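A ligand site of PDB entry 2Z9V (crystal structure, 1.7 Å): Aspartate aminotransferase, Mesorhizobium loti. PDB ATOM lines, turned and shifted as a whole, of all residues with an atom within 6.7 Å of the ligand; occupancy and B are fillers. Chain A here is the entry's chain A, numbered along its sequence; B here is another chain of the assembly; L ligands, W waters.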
ATOM      1  N   ALA A  15     -30.559 -12.652  33.890  1.00  0.00           N
ATOM      2  CA  ALA A  15     -30.859 -13.556  32.774  1.00  0.00           C
ATOM      3  C   ALA A  15     -31.157 -14.989  33.260  1.00  0.00           C
ATOM      4  O   ALA A  15     -31.005 -15.966  32.505  1.00  0.00           O
ATOM      5  CB  ALA A  15     -29.693 -13.529  31.768  1.00  0.00           C
ATOM      6  N   GLY A  16     -31.574 -15.122  34.526  1.00  0.00           N
ATOM      7  CA  GLY A  16     -32.033 -16.413  35.074  1.00  0.00           C
ATOM      8  C   GLY A  16     -31.015 -17.117  35.964  1.00  0.00           C
ATOM      9  O   GLY A  16     -29.820 -17.095  35.672  1.00  0.00           O
ATOM     10  N   GLU A  67     -31.687 -30.158  35.141  1.00  0.00           N
ATOM     11  CA  GLU A  67     -31.784 -28.934  34.363  1.00  0.00           C
ATOM     12  C   GLU A  67     -31.109 -29.156  32.987  1.00  0.00           C
ATOM     13  O   GLU A  67     -30.420 -30.161  32.781  1.00  0.00           O
ATOM     14  CB  GLU A  67     -31.315 -27.729  35.177  1.00  0.00           C
ATOM     15  CG  GLU A  67     -29.847 -27.442  35.206  1.00  0.00           C
ATOM     16  CD  GLU A  67     -29.507 -26.294  34.288  1.00  0.00           C
ATOM     17  OE1 GLU A  67     -30.085 -25.203  34.468  1.00  0.00           O
ATOM     18  OE2 GLU A  67     -28.672 -26.502  33.377  1.00  0.00           O
ATOM     19  N   PRO A  68     -31.378 -28.268  32.025  1.00  0.00           N
ATOM     20  CA  PRO A  68     -31.010 -28.538  30.630  1.00  0.00           C
ATOM     21  C   PRO A  68     -29.585 -28.910  30.257  1.00  0.00           C
ATOM     22  O   PRO A  68     -29.409 -29.510  29.189  1.00  0.00           O
ATOM     23  CB  PRO A  68     -31.435 -27.236  29.915  1.00  0.00           C
ATOM     24  CG  PRO A  68     -32.588 -26.782  30.686  1.00  0.00           C
ATOM     25  CD  PRO A  68     -32.172 -27.020  32.115  1.00  0.00           C
ATOM     26  N   VAL A  69     -28.585 -28.609  31.099  1.00  0.00           N
ATOM     27  CA  VAL A  69     -27.247 -29.176  30.838  1.00  0.00           C
ATOM     28  C   VAL A  69     -27.329 -30.690  30.655  1.00  0.00           C
ATOM     29  O   VAL A  69     -26.555 -31.256  29.881  1.00  0.00           O
ATOM     30  CB  VAL A  69     -26.202 -28.900  31.945  1.00  0.00           C
ATOM     31  CG1 VAL A  69     -25.739 -27.454  31.911  1.00  0.00           C
ATOM     32  CG2 VAL A  69     -26.704 -29.307  33.338  1.00  0.00           C
ATOM     33  N   LEU A  70     -28.251 -31.332  31.360  1.00  0.00           N
ATOM     34  CA  LEU A  70     -28.454 -32.771  31.229  1.00  0.00           C
ATOM     35  C   LEU A  70     -28.884 -33.148  29.817  1.00  0.00           C
ATOM     36  O   LEU A  70     -28.328 -34.089  29.226  1.00  0.00           O
ATOM     37  CB  LEU A  70     -29.501 -33.261  32.223  1.00  0.00           C
ATOM     38  CG  LEU A  70     -29.872 -34.747  32.136  1.00  0.00           C
ATOM     39  CD1 LEU A  70     -28.628 -35.647  32.271  1.00  0.00           C
ATOM     40  CD2 LEU A  70     -30.898 -35.095  33.210  1.00  0.00           C
ATOM     41  N   LEU A  72     -28.445 -31.464  27.038  1.00  0.00           N
ATOM     42  CA  LEU A  72     -27.378 -31.195  26.087  1.00  0.00           C
ATOM     43  C   LEU A  72     -26.284 -32.277  26.124  1.00  0.00           C
ATOM     44  O   LEU A  72     -25.887 -32.789  25.090  1.00  0.00           O
ATOM     45  CB  LEU A  72     -26.817 -29.790  26.286  1.00  0.00           C
ATOM     46  CG  LEU A  72     -27.851 -28.730  25.893  1.00  0.00           C
ATOM     47  CD1 LEU A  72     -27.476 -27.385  26.466  1.00  0.00           C
ATOM     48  CD2 LEU A  72     -28.040 -28.670  24.348  1.00  0.00           C
ATOM     49  N   TYR A  94     -21.749 -20.910  25.500  1.00  0.00           N
ATOM     50  CA  TYR A  94     -22.472 -22.185  25.401  1.00  0.00           C
ATOM     51  C   TYR A  94     -22.229 -22.920  24.088  1.00  0.00           C
ATOM     52  O   TYR A  94     -22.038 -24.137  24.071  1.00  0.00           O
ATOM     53  CB  TYR A  94     -23.953 -22.013  25.716  1.00  0.00           C
ATOM     54  CG  TYR A  94     -24.152 -21.929  27.209  1.00  0.00           C
ATOM     55  CD1 TYR A  94     -24.139 -23.085  27.993  1.00  0.00           C
ATOM     56  CD2 TYR A  94     -24.303 -20.698  27.844  1.00  0.00           C
ATOM     57  CE1 TYR A  94     -24.290 -23.003  29.383  1.00  0.00           C
ATOM     58  CE2 TYR A  94     -24.448 -20.604  29.228  1.00  0.00           C
ATOM     59  CZ  TYR A  94     -24.434 -21.752  29.981  1.00  0.00           C
ATOM     60  OH  TYR A  94     -24.572 -21.665  31.361  1.00  0.00           O
ATOM     61  N   GLY A  95     -22.244 -22.182  22.974  1.00  0.00           N
ATOM     62  CA  GLY A  95     -21.997 -22.780  21.674  1.00  0.00           C
ATOM     63  C   GLY A  95     -20.616 -23.418  21.642  1.00  0.00           C
ATOM     64  O   GLY A  95     -20.461 -24.570  21.253  1.00  0.00           O
ATOM     65  N   CYS A 141     -26.447 -23.107  19.126  1.00  0.00           N
ATOM     66  CA  CYS A 141     -27.105 -22.464  20.260  1.00  0.00           C
ATOM     67  C   CYS A 141     -27.979 -21.313  19.754  1.00  0.00           C
ATOM     68  O   CYS A 141     -27.497 -20.441  19.030  1.00  0.00           O
ATOM     69  CB  CYS A 141     -26.073 -21.935  21.248  1.00  0.00           C
ATOM     70  SG  CYS A 141     -26.769 -21.229  22.765  1.00  0.00           S
ATOM     71  N   HIS A 142     -29.248 -21.291  20.143  1.00  0.00           N
ATOM     72  CA  HIS A 142     -30.163 -20.244  19.683  1.00  0.00           C
ATOM     73  C   HIS A 142     -29.899 -18.883  20.333  1.00  0.00           C
ATOM     74  O   HIS A 142     -29.645 -17.892  19.638  1.00  0.00           O
ATOM     75  CB  HIS A 142     -31.606 -20.678  19.905  1.00  0.00           C
ATOM     76  CG  HIS A 142     -32.612 -19.817  19.220  1.00  0.00           C
ATOM     77  ND1 HIS A 142     -33.934 -19.796  19.595  1.00  0.00           N
ATOM     78  CD2 HIS A 142     -32.489 -18.937  18.185  1.00  0.00           C
ATOM     79  CE1 HIS A 142     -34.595 -18.946  18.810  1.00  0.00           C
ATOM     80  NE2 HIS A 142     -33.746 -18.414  17.948  1.00  0.00           N
ATOM     81  N   HIS A 143     -29.962 -18.841  21.663  1.00  0.00           N
ATOM     82  CA  HIS A 143     -29.630 -17.652  22.416  1.00  0.00           C
ATOM     83  C   HIS A 143     -28.435 -18.022  23.294  1.00  0.00           C
ATOM     84  O   HIS A 143     -28.583 -18.777  24.239  1.00  0.00           O
ATOM     85  CB  HIS A 143     -30.849 -17.226  23.255  1.00  0.00           C
ATOM     86  CG  HIS A 143     -30.608 -16.097  24.214  1.00  0.00           C
ATOM     87  ND1 HIS A 143     -29.644 -15.124  24.038  1.00  0.00           N
ATOM     88  CD2 HIS A 143     -31.267 -15.759  25.350  1.00  0.00           C
ATOM     89  CE1 HIS A 143     -29.704 -14.257  25.037  1.00  0.00           C
ATOM     90  NE2 HIS A 143     -30.685 -14.624  25.841  1.00  0.00           N
ATOM     91  N   ASP A 144     -27.258 -17.525  22.930  1.00  0.00           N
ATOM     92  CA  ASP A 144     -26.085 -17.815  23.763  1.00  0.00           C
ATOM     93  C   ASP A 144     -26.072 -16.801  24.893  1.00  0.00           C
ATOM     94  O   ASP A 144     -25.557 -15.700  24.773  1.00  0.00           O
ATOM     95  CB  ASP A 144     -24.789 -17.786  22.937  1.00  0.00           C
ATOM     96  CG  ASP A 144     -23.717 -18.670  23.529  1.00  0.00           C
ATOM     97  OD1 ASP A 144     -23.480 -18.561  24.750  1.00  0.00           O
ATOM     98  OD2 ASP A 144     -23.134 -19.496  22.763  1.00  0.00           O
ATOM     99  N   THR A 145     -26.718 -17.174  25.989  1.00  0.00           N
ATOM    100  CA  THR A 145     -27.177 -16.231  27.008  1.00  0.00           C
ATOM    101  C   THR A 145     -26.117 -15.239  27.532  1.00  0.00           C
ATOM    102  O   THR A 145     -26.409 -14.046  27.672  1.00  0.00           O
ATOM    103  CB  THR A 145     -27.882 -16.960  28.173  1.00  0.00           C
ATOM    104  OG1 THR A 145     -28.481 -18.162  27.674  1.00  0.00           O
ATOM    105  CG2 THR A 145     -28.976 -16.068  28.792  1.00  0.00           C
ATOM    106  N   PRO A 146     -24.886 -15.710  27.823  1.00  0.00           N
ATOM    107  CA  PRO A 146     -23.820 -14.807  28.288  1.00  0.00           C
ATOM    108  C   PRO A 146     -23.436 -13.698  27.307  1.00  0.00           C
ATOM    109  O   PRO A 146     -22.701 -12.796  27.679  1.00  0.00           O
ATOM    110  CB  PRO A 146     -22.626 -15.759  28.522  1.00  0.00           C
ATOM    111  CG  PRO A 146     -23.291 -17.090  28.840  1.00  0.00           C
ATOM    112  CD  PRO A 146     -24.442 -17.118  27.838  1.00  0.00           C
ATOM    113  N   ASP A 170     -29.713 -25.921  21.046  1.00  0.00           N
ATOM    114  CA  ASP A 170     -29.851 -25.441  22.422  1.00  0.00           C
ATOM    115  C   ASP A 170     -30.781 -24.227  22.362  1.00  0.00           C
ATOM    116  O   ASP A 170     -30.379 -23.158  21.871  1.00  0.00           O
ATOM    117  CB  ASP A 170     -28.461 -25.061  22.962  1.00  0.00           C
ATOM    118  CG  ASP A 170     -28.494 -24.294  24.293  1.00  0.00           C
ATOM    119  OD1 ASP A 170     -27.407 -24.184  24.905  1.00  0.00           O
ATOM    120  OD2 ASP A 170     -29.574 -23.811  24.733  1.00  0.00           O
ATOM    121  N   ALA A 171     -32.024 -24.394  22.807  1.00  0.00           N
ATOM    122  CA  ALA A 171     -32.946 -23.260  22.932  1.00  0.00           C
ATOM    123  C   ALA A 171     -33.358 -23.023  24.389  1.00  0.00           C
ATOM    124  O   ALA A 171     -34.485 -22.605  24.678  1.00  0.00           O
ATOM    125  CB  ALA A 171     -34.182 -23.474  22.058  1.00  0.00           C
ATOM    126  N   VAL A 172     -32.413 -23.269  25.302  1.00  0.00           N
ATOM    127  CA  VAL A 172     -32.712 -23.152  26.730  1.00  0.00           C
ATOM    128  C   VAL A 172     -33.215 -21.747  27.104  1.00  0.00           C
ATOM    129  O   VAL A 172     -34.160 -21.604  27.878  1.00  0.00           O
ATOM    130  CB  VAL A 172     -31.460 -23.521  27.563  1.00  0.00           C
ATOM    131  CG1 VAL A 172     -31.704 -23.186  29.046  1.00  0.00           C
ATOM    132  CG2 VAL A 172     -31.173 -24.997  27.369  1.00  0.00           C
ATOM    133  N   SER A 173     -32.608 -20.713  26.530  1.00  0.00           N
ATOM    134  CA  SER A 173     -32.923 -19.360  26.975  1.00  0.00           C
ATOM    135  C   SER A 173     -33.679 -18.553  25.935  1.00  0.00           C
ATOM    136  O   SER A 173     -33.741 -17.334  26.041  1.00  0.00           O
ATOM    137  CB  SER A 173     -31.635 -18.645  27.377  1.00  0.00           C
ATOM    138  OG  SER A 173     -30.733 -18.630  26.282  1.00  0.00           O
ATOM    139  N   ASN A 195     -36.845 -22.991  32.993  1.00  0.00           N
ATOM    140  CA  ASN A 195     -36.165 -22.138  33.981  1.00  0.00           C
ATOM    141  C   ASN A 195     -35.641 -20.807  33.463  1.00  0.00           C
ATOM    142  O   ASN A 195     -34.933 -20.090  34.192  1.00  0.00           O
ATOM    143  CB  ASN A 195     -35.040 -22.936  34.640  1.00  0.00           C
ATOM    144  CG  ASN A 195     -34.047 -23.462  33.636  1.00  0.00           C
ATOM    145  OD1 ASN A 195     -34.348 -24.385  32.865  1.00  0.00           O
ATOM    146  ND2 ASN A 195     -32.854 -22.854  33.613  1.00  0.00           N
ATOM    147  N   LYS A 196     -35.971 -20.478  32.213  1.00  0.00           N
ATOM    148  CA  LYS A 196     -35.633 -19.162  31.692  1.00  0.00           C
ATOM    149  C   LYS A 196     -36.960 -18.445  31.387  1.00  0.00           C
ATOM    150  O   LYS A 196     -37.629 -18.001  32.305  1.00  0.00           O
ATOM    151  CB  LYS A 196     -34.691 -19.239  30.484  1.00  0.00           C
ATOM    152  CG  LYS A 196     -33.298 -19.853  30.805  1.00  0.00           C
ATOM    153  CD  LYS A 196     -32.480 -18.962  31.739  1.00  0.00           C
ATOM    154  CE  LYS A 196     -30.985 -19.348  31.699  1.00  0.00           C
ATOM    155  NZ  LYS A 196     -30.238 -18.655  32.797  1.00  0.00           N
ATOM    156  N   ARG A 335     -20.247 -14.465  31.563  1.00  0.00           N
ATOM    157  CA  ARG A 335     -19.752 -15.803  31.890  1.00  0.00           C
ATOM    158  C   ARG A 335     -18.548 -16.093  30.987  1.00  0.00           C
ATOM    159  O   ARG A 335     -18.514 -15.641  29.840  1.00  0.00           O
ATOM    160  CB  ARG A 335     -20.868 -16.833  31.667  1.00  0.00           C
ATOM    161  CG  ARG A 335     -20.586 -18.251  32.145  1.00  0.00           C
ATOM    162  CD  ARG A 335     -21.758 -19.190  31.855  1.00  0.00           C
ATOM    163  NE  ARG A 335     -22.861 -19.046  32.810  1.00  0.00           N
ATOM    164  CZ  ARG A 335     -22.970 -19.749  33.934  1.00  0.00           C
ATOM    165  NH1 ARG A 335     -22.033 -20.634  34.266  1.00  0.00           N
ATOM    166  NH2 ARG A 335     -24.007 -19.566  34.736  1.00  0.00           N
ATOM    167  N   ARG A 344     -25.766  -8.135  32.159  1.00  0.00           N
ATOM    168  CA  ARG A 344     -26.980  -8.624  31.493  1.00  0.00           C
ATOM    169  C   ARG A 344     -28.235  -8.353  32.293  1.00  0.00           C
ATOM    170  O   ARG A 344     -28.291  -8.587  33.512  1.00  0.00           O
ATOM    171  CB  ARG A 344     -26.870 -10.116  31.177  1.00  0.00           C
ATOM    172  CG  ARG A 344     -25.764 -10.428  30.192  1.00  0.00           C
ATOM    173  CD  ARG A 344     -25.633 -11.912  29.922  1.00  0.00           C
ATOM    174  NE  ARG A 344     -25.167 -12.637  31.123  1.00  0.00           N
ATOM    175  CZ  ARG A 344     -25.514 -13.885  31.406  1.00  0.00           C
ATOM    176  NH1 ARG A 344     -26.344 -14.560  30.610  1.00  0.00           N
ATOM    177  NH2 ARG A 344     -25.046 -14.456  32.525  1.00  0.00           N
ATOM    178  N   PHE B 246     -23.019 -26.178  37.323  1.00  0.00           N
ATOM    179  CA  PHE B 246     -24.200 -25.794  36.541  1.00  0.00           C
ATOM    180  C   PHE B 246     -25.257 -25.277  37.497  1.00  0.00           C
ATOM    181  O   PHE B 246     -25.035 -25.253  38.712  1.00  0.00           O
ATOM    182  CB  PHE B 246     -24.707 -26.955  35.655  1.00  0.00           C
ATOM    183  CG  PHE B 246     -25.101 -28.200  36.408  1.00  0.00           C
ATOM    184  CD1 PHE B 246     -24.213 -29.280  36.501  1.00  0.00           C
ATOM    185  CD2 PHE B 246     -26.372 -28.331  36.970  1.00  0.00           C
ATOM    186  CE1 PHE B 246     -24.575 -30.461  37.178  1.00  0.00           C
ATOM    187  CE2 PHE B 246     -26.735 -29.508  37.637  1.00  0.00           C
ATOM    188  CZ  PHE B 246     -25.841 -30.568  37.739  1.00  0.00           C
ATOM    189  N   THR B 247     -26.407 -24.844  36.974  1.00  0.00           N
ATOM    190  CA  THR B 247     -27.381 -24.136  37.795  1.00  0.00           C
ATOM    191  C   THR B 247     -28.014 -25.058  38.844  1.00  0.00           C
ATOM    192  O   THR B 247     -28.604 -26.099  38.495  1.00  0.00           O
ATOM    193  CB  THR B 247     -28.463 -23.476  36.928  1.00  0.00           C
ATOM    194  OG1 THR B 247     -27.835 -22.711  35.890  1.00  0.00           O
ATOM    195  CG2 THR B 247     -29.330 -22.561  37.765  1.00  0.00           C
HETATM  196  N1  LIG L   1     -27.652 -23.244  27.297  1.00  0.00           N
HETATM  197  C1  LIG L   1     -27.827 -21.954  27.589  1.00  0.00           C
HETATM  198  C2  LIG L   1     -27.837 -20.972  26.417  1.00  0.00           C
HETATM  199  C3  LIG L   1     -28.012 -21.540  28.907  1.00  0.00           C
HETATM  200  O1  LIG L   1     -28.204 -20.230  29.190  1.00  0.00           O
HETATM  201  C4  LIG L   1     -28.006 -22.477  29.943  1.00  0.00           C
HETATM  202  C5  LIG L   1     -27.817 -23.828  29.571  1.00  0.00           C
HETATM  203  C6  LIG L   1     -27.779 -24.997  30.549  1.00  0.00           C
HETATM  204  O2  LIG L   1     -29.042 -25.075  31.193  1.00  0.00           O
HETATM  205  C7  LIG L   1     -27.642 -24.169  28.235  1.00  0.00           C
HETATM  206  C8  LIG L   1     -28.206 -22.046  31.399  1.00  0.00           C
HETATM  207  N2  LIG L   1     -27.269 -20.949  31.705  1.00  0.00           N
HETATM  208  O   HOH W   1     -29.230 -20.936  34.453  1.00  0.00           O
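The side-chain hydroxyl (OG1) of Thr 145 sits at hydrogen-bond distance from an oxygen (O1) of the ligand, 2.6 Å away. A nitrogen (N1) of the ligand lies within hydrogen-bond range of the side-chain carboxylate (OD1) of Asp 170, at 2.6 Å. OE2 of Glu 67 lies within hydrogen-bond range of O2 of the ligand, 2.6 Å away. The side-chain hydroxyl (OH) of Tyr 94 sits at hydrogen-bond distance from a nitrogen (N2) of the ligand (2.8 Å).
O of His 143 sits at hydrogen-bond distance from OG1 of Thr 145, at 3.5 Å. The side-chain hydroxyl of Ser 173 sits at hydrogen-bond distance from the side-chain hydroxyl of Thr 145, at 2.7 Å. The backbone carbonyl oxygen of Thr 145 sits at hydrogen-bond distance from the guanidinium group of Arg 344, at 3.0 Å. SG of Cys 141 lies within hydrogen-bond range of OD1 of Asp 170, 3.7 Å away. OE2 of Glu 67 sits at hydrogen-bond distance from N of Val 69, 3.1 Å away. SG of Cys 141 lies within hydrogen-bond range of O of His 143, at 3.4 Å. SG of Cys 141 sits close to N of Asp 144 (3.7 Å). The backbone carbonyl oxygen of Gly 16 lies within hydrogen-bond range of the side-chain amino group of Lys 196 (3.3 Å).
Pro 68 touches the ligand (CB to O2, 3.5 Å). CG1 of Val 69 touches C6 of the ligand, 3.5 Å away. CD1 of Leu 72 touches C7 of the ligand, at 3.7 Å. Cys 141 touches the ligand. His 143 touches the ligand (O to C2, 3.2 Å). CG2 of Val 172 touches C7 of the ligand, 3.7 Å away. Ser 173 touches the ligand. Lys 196 touches the ligand. Within 4 Å of the ligand: Glu 67, Pro 68, Val 69, Leu 72, Tyr 94, Cys 141, His 143, Thr 145, Asp 170, Val 172, Ser 173 and Lys 196.
Water W1 lies within hydrogen-bond range of OG1 of Thr 247 of chain B, NZ of Lys 196 and N2 of the ligand.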
